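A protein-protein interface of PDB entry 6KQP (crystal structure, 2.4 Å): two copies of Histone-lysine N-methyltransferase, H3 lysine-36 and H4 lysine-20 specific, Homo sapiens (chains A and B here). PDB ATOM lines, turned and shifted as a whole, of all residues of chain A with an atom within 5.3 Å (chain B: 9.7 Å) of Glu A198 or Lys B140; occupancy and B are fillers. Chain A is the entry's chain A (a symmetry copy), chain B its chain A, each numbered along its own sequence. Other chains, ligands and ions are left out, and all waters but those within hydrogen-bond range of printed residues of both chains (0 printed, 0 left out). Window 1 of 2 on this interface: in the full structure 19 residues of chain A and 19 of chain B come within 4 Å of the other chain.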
ATOM      1  N   MET A 135      -2.954 -22.397 -28.208  1.00  0.00           N
ATOM      2  CA  MET A 135      -2.051 -23.069 -29.171  1.00  0.00           C
ATOM      3  C   MET A 135      -0.724 -23.393 -28.487  1.00  0.00           C
ATOM      4  O   MET A 135      -0.134 -22.496 -27.894  1.00  0.00           O
ATOM      5  CB  MET A 135      -1.842 -22.173 -30.388  1.00  0.00           C
ATOM      6  CG  MET A 135      -3.151 -21.939 -31.091  1.00  0.00           C
ATOM      7  SD  MET A 135      -3.009 -22.183 -32.831  1.00  0.00           S
ATOM      8  CE  MET A 135      -4.682 -21.834 -33.358  1.00  0.00           C
ATOM      9  N   LEU A 136      -0.333 -24.658 -28.514  1.00  0.00           N
ATOM     10  CA  LEU A 136       0.852 -25.166 -27.787  1.00  0.00           C
ATOM     11  C   LEU A 136       1.499 -26.213 -28.680  1.00  0.00           C
ATOM     12  O   LEU A 136       0.785 -27.143 -29.099  1.00  0.00           O
ATOM     13  CB  LEU A 136       0.399 -25.752 -26.448  1.00  0.00           C
ATOM     14  CG  LEU A 136       1.516 -26.055 -25.455  1.00  0.00           C
ATOM     15  CD1 LEU A 136       1.045 -25.822 -24.030  1.00  0.00           C
ATOM     16  CD2 LEU A 136       2.004 -27.486 -25.618  1.00  0.00           C
ATOM     17  N   THR A 137       2.779 -26.017 -28.996  1.00  0.00           N
ATOM     18  CA  THR A 137       3.496 -26.764 -30.051  1.00  0.00           C
ATOM     19  C   THR A 137       3.737 -28.154 -29.483  1.00  0.00           C
ATOM     20  O   THR A 137       4.216 -28.232 -28.338  1.00  0.00           O
ATOM     21  CB  THR A 137       4.768 -26.027 -30.494  1.00  0.00           C
ATOM     22  OG1 THR A 137       5.642 -25.959 -29.372  1.00  0.00           O
ATOM     23  CG2 THR A 137       4.528 -24.613 -30.972  1.00  0.00           C
ATOM     24  N   GLU A 165       4.641 -27.364 -14.598  1.00  0.00           N
ATOM     25  CA  GLU A 165       5.439 -27.322 -15.852  1.00  0.00           C
ATOM     26  C   GLU A 165       4.835 -28.294 -16.856  1.00  0.00           C
ATOM     27  O   GLU A 165       4.119 -29.225 -16.446  1.00  0.00           O
ATOM     28  CB  GLU A 165       6.894 -27.672 -15.577  1.00  0.00           C
ATOM     29  CG  GLU A 165       7.113 -29.140 -15.231  1.00  0.00           C
ATOM     30  CD  GLU A 165       8.570 -29.540 -15.011  1.00  0.00           C
ATOM     31  OE1 GLU A 165       9.476 -28.727 -15.316  1.00  0.00           O
ATOM     32  OE2 GLU A 165       8.801 -30.675 -14.520  1.00  0.00           O
ATOM     33  N   THR A 166       5.137 -28.094 -18.125  1.00  0.00           N
ATOM     34  CA  THR A 166       4.816 -29.071 -19.193  1.00  0.00           C
ATOM     35  C   THR A 166       5.910 -30.114 -19.243  1.00  0.00           C
ATOM     36  O   THR A 166       7.051 -29.780 -18.983  1.00  0.00           O
ATOM     37  CB  THR A 166       4.706 -28.427 -20.572  1.00  0.00           C
ATOM     38  OG1 THR A 166       5.994 -27.870 -20.867  1.00  0.00           O
ATOM     39  CG2 THR A 166       3.608 -27.395 -20.590  1.00  0.00           C
ATOM     40  N   GLN A 167       5.546 -31.330 -19.580  1.00  0.00           N
ATOM     41  CA  GLN A 167       6.508 -32.405 -19.911  1.00  0.00           C
ATOM     42  C   GLN A 167       5.935 -33.115 -21.132  1.00  0.00           C
ATOM     43  O   GLN A 167       4.728 -33.439 -21.102  1.00  0.00           O
ATOM     44  CB  GLN A 167       6.663 -33.352 -18.724  1.00  0.00           C
ATOM     45  CG  GLN A 167       7.365 -32.754 -17.513  1.00  0.00           C
ATOM     46  CD  GLN A 167       7.431 -33.753 -16.371  1.00  0.00           C
ATOM     47  OE1 GLN A 167       7.088 -34.927 -16.521  1.00  0.00           O
ATOM     48  NE2 GLN A 167       7.830 -33.297 -15.195  1.00  0.00           N
ATOM     49  N   LYS A 168       6.755 -33.331 -22.154  1.00  0.00           N
ATOM     50  CA  LYS A 168       6.362 -34.127 -23.344  1.00  0.00           C
ATOM     51  C   LYS A 168       6.639 -35.617 -23.082  1.00  0.00           C
ATOM     52  O   LYS A 168       7.794 -36.001 -22.964  1.00  0.00           O
ATOM     53  CB  LYS A 168       7.031 -33.553 -24.588  1.00  0.00           C
ATOM     54  CG  LYS A 168       6.297 -32.332 -25.113  1.00  0.00           C
ATOM     55  CD  LYS A 168       7.133 -31.482 -26.023  1.00  0.00           C
ATOM     56  CE  LYS A 168       6.356 -30.317 -26.608  1.00  0.00           C
ATOM     57  NZ  LYS A 168       7.119 -29.676 -27.709  1.00  0.00           N
ATOM     58  N   PHE A 193       1.435 -22.352 -15.461  1.00  0.00           N
ATOM     59  CA  PHE A 193       2.758 -22.797 -15.936  1.00  0.00           C
ATOM     60  C   PHE A 193       3.361 -21.710 -16.797  1.00  0.00           C
ATOM     61  O   PHE A 193       2.633 -20.850 -17.249  1.00  0.00           O
ATOM     62  CB  PHE A 193       2.656 -24.121 -16.688  1.00  0.00           C
ATOM     63  CG  PHE A 193       1.989 -24.052 -18.040  1.00  0.00           C
ATOM     64  CD1 PHE A 193       0.609 -24.102 -18.168  1.00  0.00           C
ATOM     65  CD2 PHE A 193       2.750 -24.030 -19.190  1.00  0.00           C
ATOM     66  CE1 PHE A 193       0.009 -24.115 -19.421  1.00  0.00           C
ATOM     67  CE2 PHE A 193       2.159 -24.043 -20.446  1.00  0.00           C
ATOM     68  CZ  PHE A 193       0.788 -24.096 -20.562  1.00  0.00           C
ATOM     69  N   ASN A 194       4.673 -21.759 -16.965  1.00  0.00           N
ATOM     70  CA  ASN A 194       5.418 -20.834 -17.834  1.00  0.00           C
ATOM     71  C   ASN A 194       5.274 -21.328 -19.276  1.00  0.00           C
ATOM     72  O   ASN A 194       5.678 -22.451 -19.549  1.00  0.00           O
ATOM     73  CB  ASN A 194       6.887 -20.796 -17.439  1.00  0.00           C
ATOM     74  CG  ASN A 194       7.645 -19.652 -18.077  1.00  0.00           C
ATOM     75  OD1 ASN A 194       7.373 -19.245 -19.212  1.00  0.00           O
ATOM     76  ND2 ASN A 194       8.616 -19.140 -17.346  1.00  0.00           N
ATOM     77  N   TYR A 195       4.735 -20.493 -20.161  1.00  0.00           N
ATOM     78  CA  TYR A 195       4.460 -20.828 -21.577  1.00  0.00           C
ATOM     79  C   TYR A 195       5.782 -21.039 -22.309  1.00  0.00           C
ATOM     80  O   TYR A 195       5.794 -21.812 -23.285  1.00  0.00           O
ATOM     81  CB  TYR A 195       3.606 -19.732 -22.226  1.00  0.00           C
ATOM     82  CG  TYR A 195       2.162 -19.718 -21.791  1.00  0.00           C
ATOM     83  CD1 TYR A 195       1.699 -20.560 -20.787  1.00  0.00           C
ATOM     84  CD2 TYR A 195       1.258 -18.844 -22.370  1.00  0.00           C
ATOM     85  CE1 TYR A 195       0.377 -20.538 -20.375  1.00  0.00           C
ATOM     86  CE2 TYR A 195      -0.072 -18.824 -21.987  1.00  0.00           C
ATOM     87  CZ  TYR A 195      -0.509 -19.668 -20.985  1.00  0.00           C
ATOM     88  OH  TYR A 195      -1.812 -19.677 -20.584  1.00  0.00           O
ATOM     89  N   ASN A 196       6.846 -20.373 -21.856  1.00  0.00           N
ATOM     90  CA  ASN A 196       8.197 -20.450 -22.481  1.00  0.00           C
ATOM     91  C   ASN A 196       8.045 -20.242 -23.991  1.00  0.00           C
ATOM     92  O   ASN A 196       7.303 -19.313 -24.364  1.00  0.00           O
ATOM     93  CB  ASN A 196       8.898 -21.752 -22.098  1.00  0.00           C
ATOM     94  CG  ASN A 196       9.501 -21.734 -20.702  1.00  0.00           C
ATOM     95  OD1 ASN A 196       9.150 -22.577 -19.870  1.00  0.00           O
ATOM     96  ND2 ASN A 196      10.417 -20.807 -20.434  1.00  0.00           N
ATOM     97  N   LEU A 197       8.679 -21.084 -24.821  1.00  0.00           N
ATOM     98  CA  LEU A 197       8.650 -21.003 -26.306  1.00  0.00           C
ATOM     99  C   LEU A 197       7.449 -21.763 -26.887  1.00  0.00           C
ATOM    100  O   LEU A 197       7.307 -21.716 -28.108  1.00  0.00           O
ATOM    101  CB  LEU A 197       9.935 -21.611 -26.874  1.00  0.00           C
ATOM    102  CG  LEU A 197      11.253 -21.075 -26.314  1.00  0.00           C
ATOM    103  CD1 LEU A 197      12.433 -21.974 -26.692  1.00  0.00           C
ATOM    104  CD2 LEU A 197      11.492 -19.638 -26.773  1.00  0.00           C
ATOM    105  N   GLU A 198       6.630 -22.434 -26.066  1.00  0.00           N
ATOM    106  CA  GLU A 198       5.700 -23.515 -26.500  1.00  0.00           C
ATOM    107  C   GLU A 198       4.363 -22.952 -27.001  1.00  0.00           C
ATOM    108  O   GLU A 198       3.750 -23.590 -27.832  1.00  0.00           O
ATOM    109  CB  GLU A 198       5.420 -24.479 -25.346  1.00  0.00           C
ATOM    110  CG  GLU A 198       6.629 -25.284 -24.929  1.00  0.00           C
ATOM    111  CD  GLU A 198       6.309 -26.516 -24.092  1.00  0.00           C
ATOM    112  OE1 GLU A 198       5.623 -26.368 -23.052  1.00  0.00           O
ATOM    113  OE2 GLU A 198       6.752 -27.613 -24.467  1.00  0.00           O
ATOM    114  N   CYS A 199       3.887 -21.837 -26.460  1.00  0.00           N
ATOM    115  CA  CYS A 199       2.569 -21.250 -26.809  1.00  0.00           C
ATOM    116  C   CYS A 199       2.731 -20.237 -27.937  1.00  0.00           C
ATOM    117  O   CYS A 199       3.799 -19.632 -28.019  1.00  0.00           O
ATOM    118  CB  CYS A 199       1.899 -20.624 -25.600  1.00  0.00           C
ATOM    119  SG  CYS A 199       1.435 -21.918 -24.422  1.00  0.00           S
ATOM    120  N   LEU A 200       1.735 -20.136 -28.820  1.00  0.00           N
ATOM    121  CA  LEU A 200       1.816 -19.257 -30.010  1.00  0.00           C
ATOM    122  C   LEU A 200       0.681 -18.237 -29.962  1.00  0.00           C
ATOM    123  O   LEU A 200      -0.341 -18.521 -29.331  1.00  0.00           O
ATOM    124  CB  LEU A 200       1.753 -20.088 -31.291  1.00  0.00           C
ATOM    125  CG  LEU A 200       2.719 -21.264 -31.379  1.00  0.00           C
ATOM    126  CD1 LEU A 200       2.389 -22.111 -32.594  1.00  0.00           C
ATOM    127  CD2 LEU A 200       4.167 -20.799 -31.435  1.00  0.00           C
ATOM    128  N   PHE B  22      21.806 -31.217 -18.911  1.00  0.00           N
ATOM    129  CA  PHE B  22      21.605 -32.465 -18.146  1.00  0.00           C
ATOM    130  C   PHE B  22      22.588 -33.511 -18.671  1.00  0.00           C
ATOM    131  O   PHE B  22      23.150 -33.360 -19.764  1.00  0.00           O
ATOM    132  CB  PHE B  22      20.136 -32.881 -18.164  1.00  0.00           C
ATOM    133  CG  PHE B  22      19.187 -31.722 -17.986  1.00  0.00           C
ATOM    134  CD1 PHE B  22      18.763 -31.319 -16.726  1.00  0.00           C
ATOM    135  CD2 PHE B  22      18.746 -31.013 -19.093  1.00  0.00           C
ATOM    136  CE1 PHE B  22      17.897 -30.246 -16.582  1.00  0.00           C
ATOM    137  CE2 PHE B  22      17.891 -29.937 -18.946  1.00  0.00           C
ATOM    138  CZ  PHE B  22      17.466 -29.555 -17.692  1.00  0.00           C
ATOM    139  N   ILE B 113      21.547 -21.281 -25.452  1.00  0.00           N
ATOM    140  CA  ILE B 113      21.180 -19.957 -24.892  1.00  0.00           C
ATOM    141  C   ILE B 113      19.708 -20.014 -24.513  1.00  0.00           C
ATOM    142  O   ILE B 113      19.040 -20.933 -25.011  1.00  0.00           O
ATOM    143  CB  ILE B 113      21.485 -18.844 -25.912  1.00  0.00           C
ATOM    144  CG1 ILE B 113      20.650 -18.988 -27.185  1.00  0.00           C
ATOM    145  CG2 ILE B 113      22.977 -18.785 -26.205  1.00  0.00           C
ATOM    146  CD1 ILE B 113      20.938 -17.935 -28.215  1.00  0.00           C
ATOM    147  N   ASP B 114      19.247 -19.077 -23.682  1.00  0.00           N
ATOM    148  CA  ASP B 114      17.838 -19.007 -23.211  1.00  0.00           C
ATOM    149  C   ASP B 114      17.080 -17.962 -24.033  1.00  0.00           C
ATOM    150  O   ASP B 114      17.719 -17.325 -24.910  1.00  0.00           O
ATOM    151  CB  ASP B 114      17.772 -18.718 -21.712  1.00  0.00           C
ATOM    152  CG  ASP B 114      18.591 -17.517 -21.270  1.00  0.00           C
ATOM    153  OD1 ASP B 114      18.621 -16.504 -22.016  1.00  0.00           O
ATOM    154  OD2 ASP B 114      19.210 -17.616 -20.192  1.00  0.00           O
ATOM    155  N   GLU B 115      15.779 -17.809 -23.763  1.00  0.00           N
ATOM    156  CA  GLU B 115      14.855 -16.903 -24.502  1.00  0.00           C
ATOM    157  C   GLU B 115      15.418 -15.474 -24.501  1.00  0.00           C
ATOM    158  O   GLU B 115      15.406 -14.807 -25.570  1.00  0.00           O
ATOM    159  CB  GLU B 115      13.455 -16.930 -23.878  1.00  0.00           C
ATOM    160  N   LEU B 136      17.860 -22.518 -33.397  1.00  0.00           N
ATOM    161  CA  LEU B 136      17.028 -23.730 -33.564  1.00  0.00           C
ATOM    162  C   LEU B 136      16.698 -24.231 -32.167  1.00  0.00           C
ATOM    163  O   LEU B 136      17.643 -24.429 -31.380  1.00  0.00           O
ATOM    164  CB  LEU B 136      17.813 -24.763 -34.375  1.00  0.00           C
ATOM    165  CG  LEU B 136      17.001 -25.950 -34.883  1.00  0.00           C
ATOM    166  CD1 LEU B 136      17.520 -26.417 -36.232  1.00  0.00           C
ATOM    167  CD2 LEU B 136      17.041 -27.093 -33.881  1.00  0.00           C
ATOM    168  N   THR B 137      15.405 -24.364 -31.871  1.00  0.00           N
ATOM    169  CA  THR B 137      14.885 -24.576 -30.504  1.00  0.00           C
ATOM    170  C   THR B 137      15.224 -26.015 -30.150  1.00  0.00           C
ATOM    171  O   THR B 137      14.942 -26.893 -30.984  1.00  0.00           O
ATOM    172  CB  THR B 137      13.392 -24.232 -30.412  1.00  0.00           C
ATOM    173  OG1 THR B 137      12.688 -25.130 -31.264  1.00  0.00           O
ATOM    174  CG2 THR B 137      13.053 -22.826 -30.853  1.00  0.00           C
ATOM    175  N   LEU B 138      15.888 -26.211 -29.013  1.00  0.00           N
ATOM    176  CA  LEU B 138      16.317 -27.537 -28.497  1.00  0.00           C
ATOM    177  C   LEU B 138      15.158 -28.199 -27.755  1.00  0.00           C
ATOM    178  O   LEU B 138      14.816 -29.357 -28.050  1.00  0.00           O
ATOM    179  CB  LEU B 138      17.516 -27.347 -27.569  1.00  0.00           C
ATOM    180  CG  LEU B 138      18.144 -28.655 -27.117  1.00  0.00           C
ATOM    181  CD1 LEU B 138      18.451 -29.527 -28.316  1.00  0.00           C
ATOM    182  CD2 LEU B 138      19.384 -28.406 -26.288  1.00  0.00           C
ATOM    183  N   ASP B 139      14.597 -27.480 -26.794  1.00  0.00           N
ATOM    184  CA  ASP B 139      13.436 -27.949 -25.995  1.00  0.00           C
ATOM    185  C   ASP B 139      12.699 -26.684 -25.571  1.00  0.00           C
ATOM    186  O   ASP B 139      13.007 -25.606 -26.164  1.00  0.00           O
ATOM    187  CB  ASP B 139      13.894 -28.821 -24.826  1.00  0.00           C
ATOM    188  CG  ASP B 139      14.870 -28.104 -23.905  1.00  0.00           C
ATOM    189  OD1 ASP B 139      15.077 -26.882 -24.073  1.00  0.00           O
ATOM    190  OD2 ASP B 139      15.436 -28.772 -23.041  1.00  0.00           O
ATOM    191  N   LYS B 140      11.851 -26.778 -24.546  1.00  0.00           N
ATOM    192  CA  LYS B 140      10.893 -25.706 -24.195  1.00  0.00           C
ATOM    193  C   LYS B 140      11.625 -24.407 -23.821  1.00  0.00           C
ATOM    194  O   LYS B 140      10.975 -23.390 -23.955  1.00  0.00           O
ATOM    195  CB  LYS B 140       9.903 -26.165 -23.111  1.00  0.00           C
ATOM    196  CG  LYS B 140      10.373 -26.074 -21.664  1.00  0.00           C
ATOM    197  CD  LYS B 140       9.434 -26.751 -20.692  1.00  0.00           C
ATOM    198  CE  LYS B 140      10.127 -27.175 -19.426  1.00  0.00           C
ATOM    199  NZ  LYS B 140       9.253 -28.065 -18.634  1.00  0.00           N
ATOM    200  N   ASP B 141      12.892 -24.419 -23.366  1.00  0.00           N
ATOM    201  CA  ASP B 141      13.568 -23.199 -22.834  1.00  0.00           C
ATOM    202  C   ASP B 141      15.054 -23.111 -23.213  1.00  0.00           C
ATOM    203  O   ASP B 141      15.777 -22.261 -22.634  1.00  0.00           O
ATOM    204  CB  ASP B 141      13.419 -23.119 -21.307  1.00  0.00           C
ATOM    205  CG  ASP B 141      13.873 -24.364 -20.552  1.00  0.00           C
ATOM    206  OD1 ASP B 141      14.675 -25.137 -21.104  1.00  0.00           O
ATOM    207  OD2 ASP B 141      13.383 -24.569 -19.429  1.00  0.00           O
ATOM    208  N   ARG B 142      15.528 -23.905 -24.163  1.00  0.00           N
ATOM    209  CA  ARG B 142      16.934 -23.805 -24.638  1.00  0.00           C
ATOM    210  C   ARG B 142      16.944 -23.746 -26.163  1.00  0.00           C
ATOM    211  O   ARG B 142      16.103 -24.412 -26.789  1.00  0.00           O
ATOM    212  CB  ARG B 142      17.758 -24.985 -24.130  1.00  0.00           C
ATOM    213  CG  ARG B 142      17.850 -25.048 -22.615  1.00  0.00           C
ATOM    214  CD  ARG B 142      18.818 -26.136 -22.199  1.00  0.00           C
ATOM    215  NE  ARG B 142      18.274 -27.446 -22.509  1.00  0.00           N
ATOM    216  CZ  ARG B 142      18.927 -28.593 -22.429  1.00  0.00           C
ATOM    217  NH1 ARG B 142      20.197 -28.625 -22.062  1.00  0.00           N
ATOM    218  NH2 ARG B 142      18.294 -29.705 -22.753  1.00  0.00           N
ATOM    219  N   ILE B 143      17.879 -22.982 -26.718  1.00  0.00           N
ATOM    220  CA  ILE B 143      17.971 -22.681 -28.171  1.00  0.00           C
ATOM    221  C   ILE B 143      19.419 -22.889 -28.566  1.00  0.00           C
ATOM    222  O   ILE B 143      20.306 -22.348 -27.859  1.00  0.00           O
ATOM    223  CB  ILE B 143      17.507 -21.245 -28.489  1.00  0.00           C
ATOM    224  CG1 ILE B 143      16.046 -21.026 -28.087  1.00  0.00           C
ATOM    225  CG2 ILE B 143      17.732 -20.922 -29.963  1.00  0.00           C
ATOM    226  CD1 ILE B 143      15.759 -19.653 -27.554  1.00  0.00           C
ATOM    227  N   LYS B 168      15.130 -35.093 -32.836  1.00  0.00           N
ATOM    228  CA  LYS B 168      15.640 -34.868 -31.459  1.00  0.00           C
ATOM    229  C   LYS B 168      15.946 -36.221 -30.796  1.00  0.00           C
ATOM    230  O   LYS B 168      15.027 -36.985 -30.540  1.00  0.00           O
ATOM    231  CB  LYS B 168      14.670 -33.975 -30.694  1.00  0.00           C
ATOM    232  CG  LYS B 168      14.853 -32.509 -31.043  1.00  0.00           C
ATOM    233  CD  LYS B 168      13.669 -31.660 -30.687  1.00  0.00           C
ATOM    234  CE  LYS B 168      13.904 -30.187 -30.961  1.00  0.00           C
ATOM    235  NZ  LYS B 168      12.841 -29.359 -30.339  1.00  0.00           N
ATOM    236  N   THR B 175      19.370 -33.753 -24.878  1.00  0.00           N
ATOM    237  CA  THR B 175      18.802 -33.684 -26.231  1.00  0.00           C
ATOM    238  C   THR B 175      19.888 -33.210 -27.176  1.00  0.00           C
ATOM    239  O   THR B 175      20.672 -32.321 -26.773  1.00  0.00           O
ATOM    240  CB  THR B 175      17.567 -32.794 -26.290  1.00  0.00           C
ATOM    241  OG1 THR B 175      16.719 -33.266 -25.250  1.00  0.00           O
ATOM    242  CG2 THR B 175      16.879 -32.879 -27.633  1.00  0.00           C
ATOM    243  N   LEU B 197       8.661 -25.181 -37.386  1.00  0.00           N
ATOM    244  CA  LEU B 197       8.486 -24.268 -36.225  1.00  0.00           C
ATOM    245  C   LEU B 197       9.803 -24.073 -35.461  1.00  0.00           C
ATOM    246  O   LEU B 197       9.775 -23.295 -34.509  1.00  0.00           O
ATOM    247  CB  LEU B 197       7.447 -24.856 -35.268  1.00  0.00           C
ATOM    248  CG  LEU B 197       6.098 -25.247 -35.875  1.00  0.00           C
ATOM    249  CD1 LEU B 197       5.282 -26.121 -34.920  1.00  0.00           C
ATOM    250  CD2 LEU B 197       5.310 -24.006 -36.289  1.00  0.00           C
ATOM    251  N   LEU B 200      14.293 -19.728 -35.473  1.00  0.00           N
ATOM    252  CA  LEU B 200      13.764 -18.430 -34.993  1.00  0.00           C
ATOM    253  C   LEU B 200      14.458 -17.294 -35.742  1.00  0.00           C
ATOM    254  O   LEU B 200      15.580 -17.498 -36.215  1.00  0.00           O
ATOM    255  CB  LEU B 200      13.970 -18.296 -33.484  1.00  0.00           C
ATOM    256  CG  LEU B 200      13.485 -19.464 -32.633  1.00  0.00           C
ATOM    257  CD1 LEU B 200      13.952 -19.285 -31.200  1.00  0.00           C
ATOM    258  CD2 LEU B 200      11.971 -19.605 -32.682  1.00  0.00           C
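NZ of Lys B140 is in salt-bridge range of OE1 of Glu A165 (3.4 Å). O of Lys B140 lies close to N of Leu A197 (3.4 Å). O of Thr A166 lies within hydrogen-bond range of NZ of Lys B140 (2.8 Å).
O of Glu A198 is in hydrogen-bond range of N of Thr A137, 2.9 Å away. The side-chain carboxylate of Glu A198 is in hydrogen-bond range of the side-chain hydroxyl of Thr A166 (2.7 Å). O of Ile B113 lies within hydrogen-bond range of N of Ile B143, 2.9 Å away. The side-chain carboxylate (OE2) of Glu A165 sits at hydrogen-bond distance from the side-chain amide nitrogen (NE2) of Gln A167 (2.9 Å). NH2 of Arg B142 lies within salt-bridge range of OD2 of Asp B139 (3.0 Å). N of Asn A196 lies within hydrogen-bond range of OD1 of Asn A194 (2.9 Å).
CB of Asn A196 touches O of Lys B140 (3.2 Å). Asn A196 touches Asp B141. Asp B139 touches Leu A197. Leu A197 touches Ile B143 (CD1 to CG1, 3.99 Å). Glu A198 touches Lys B140 (OE2 to CB, 3.7 Å).
Leu A136 touches none of the printed residues of chain B. Thr A166 touches just one residue of chain B: Lys B140. Asn A196 touches just these residues of chain B: Lys B140 (3.2 Å) and Asp B141 (3.9 Å). No residue of chain B comes within 4 Å of Cys A199. Of the printed residues of chain B, Leu A197 touches Asp B139, Lys B140 and Ile B143. Of the printed residues of chain A, Ile B143 touches Leu A197. Of the printed residues of chain A, Asp B139 touches Leu A197. Of the printed residues of chain A, Asp B141 touches Asn A196. Asn A194 touches none of the printed residues of chain B. Asp B114 touches none of the printed residues of chain A. The nearest residue of chain B that does not touch Glu A198 is Asp B139 (6.1 Å).
Printed residues of chain B that touch a printed residue of chain A: Asp B139, Lys B140, Asp B141 and Ile B143. Along chain B the printed residues that touch a printed residue of chain A span positions 139 to 143. Of the 15 printed residues of chain A, 5 touch a printed residue of chain B. Hydrophobic or aromatic side chains of chain A that line the printed part of chain B: Leu A197. Among the printed residues, 8 pairs touch across the chains.
Positions printed for both chains: 136, 137, 168, 197 and 200.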
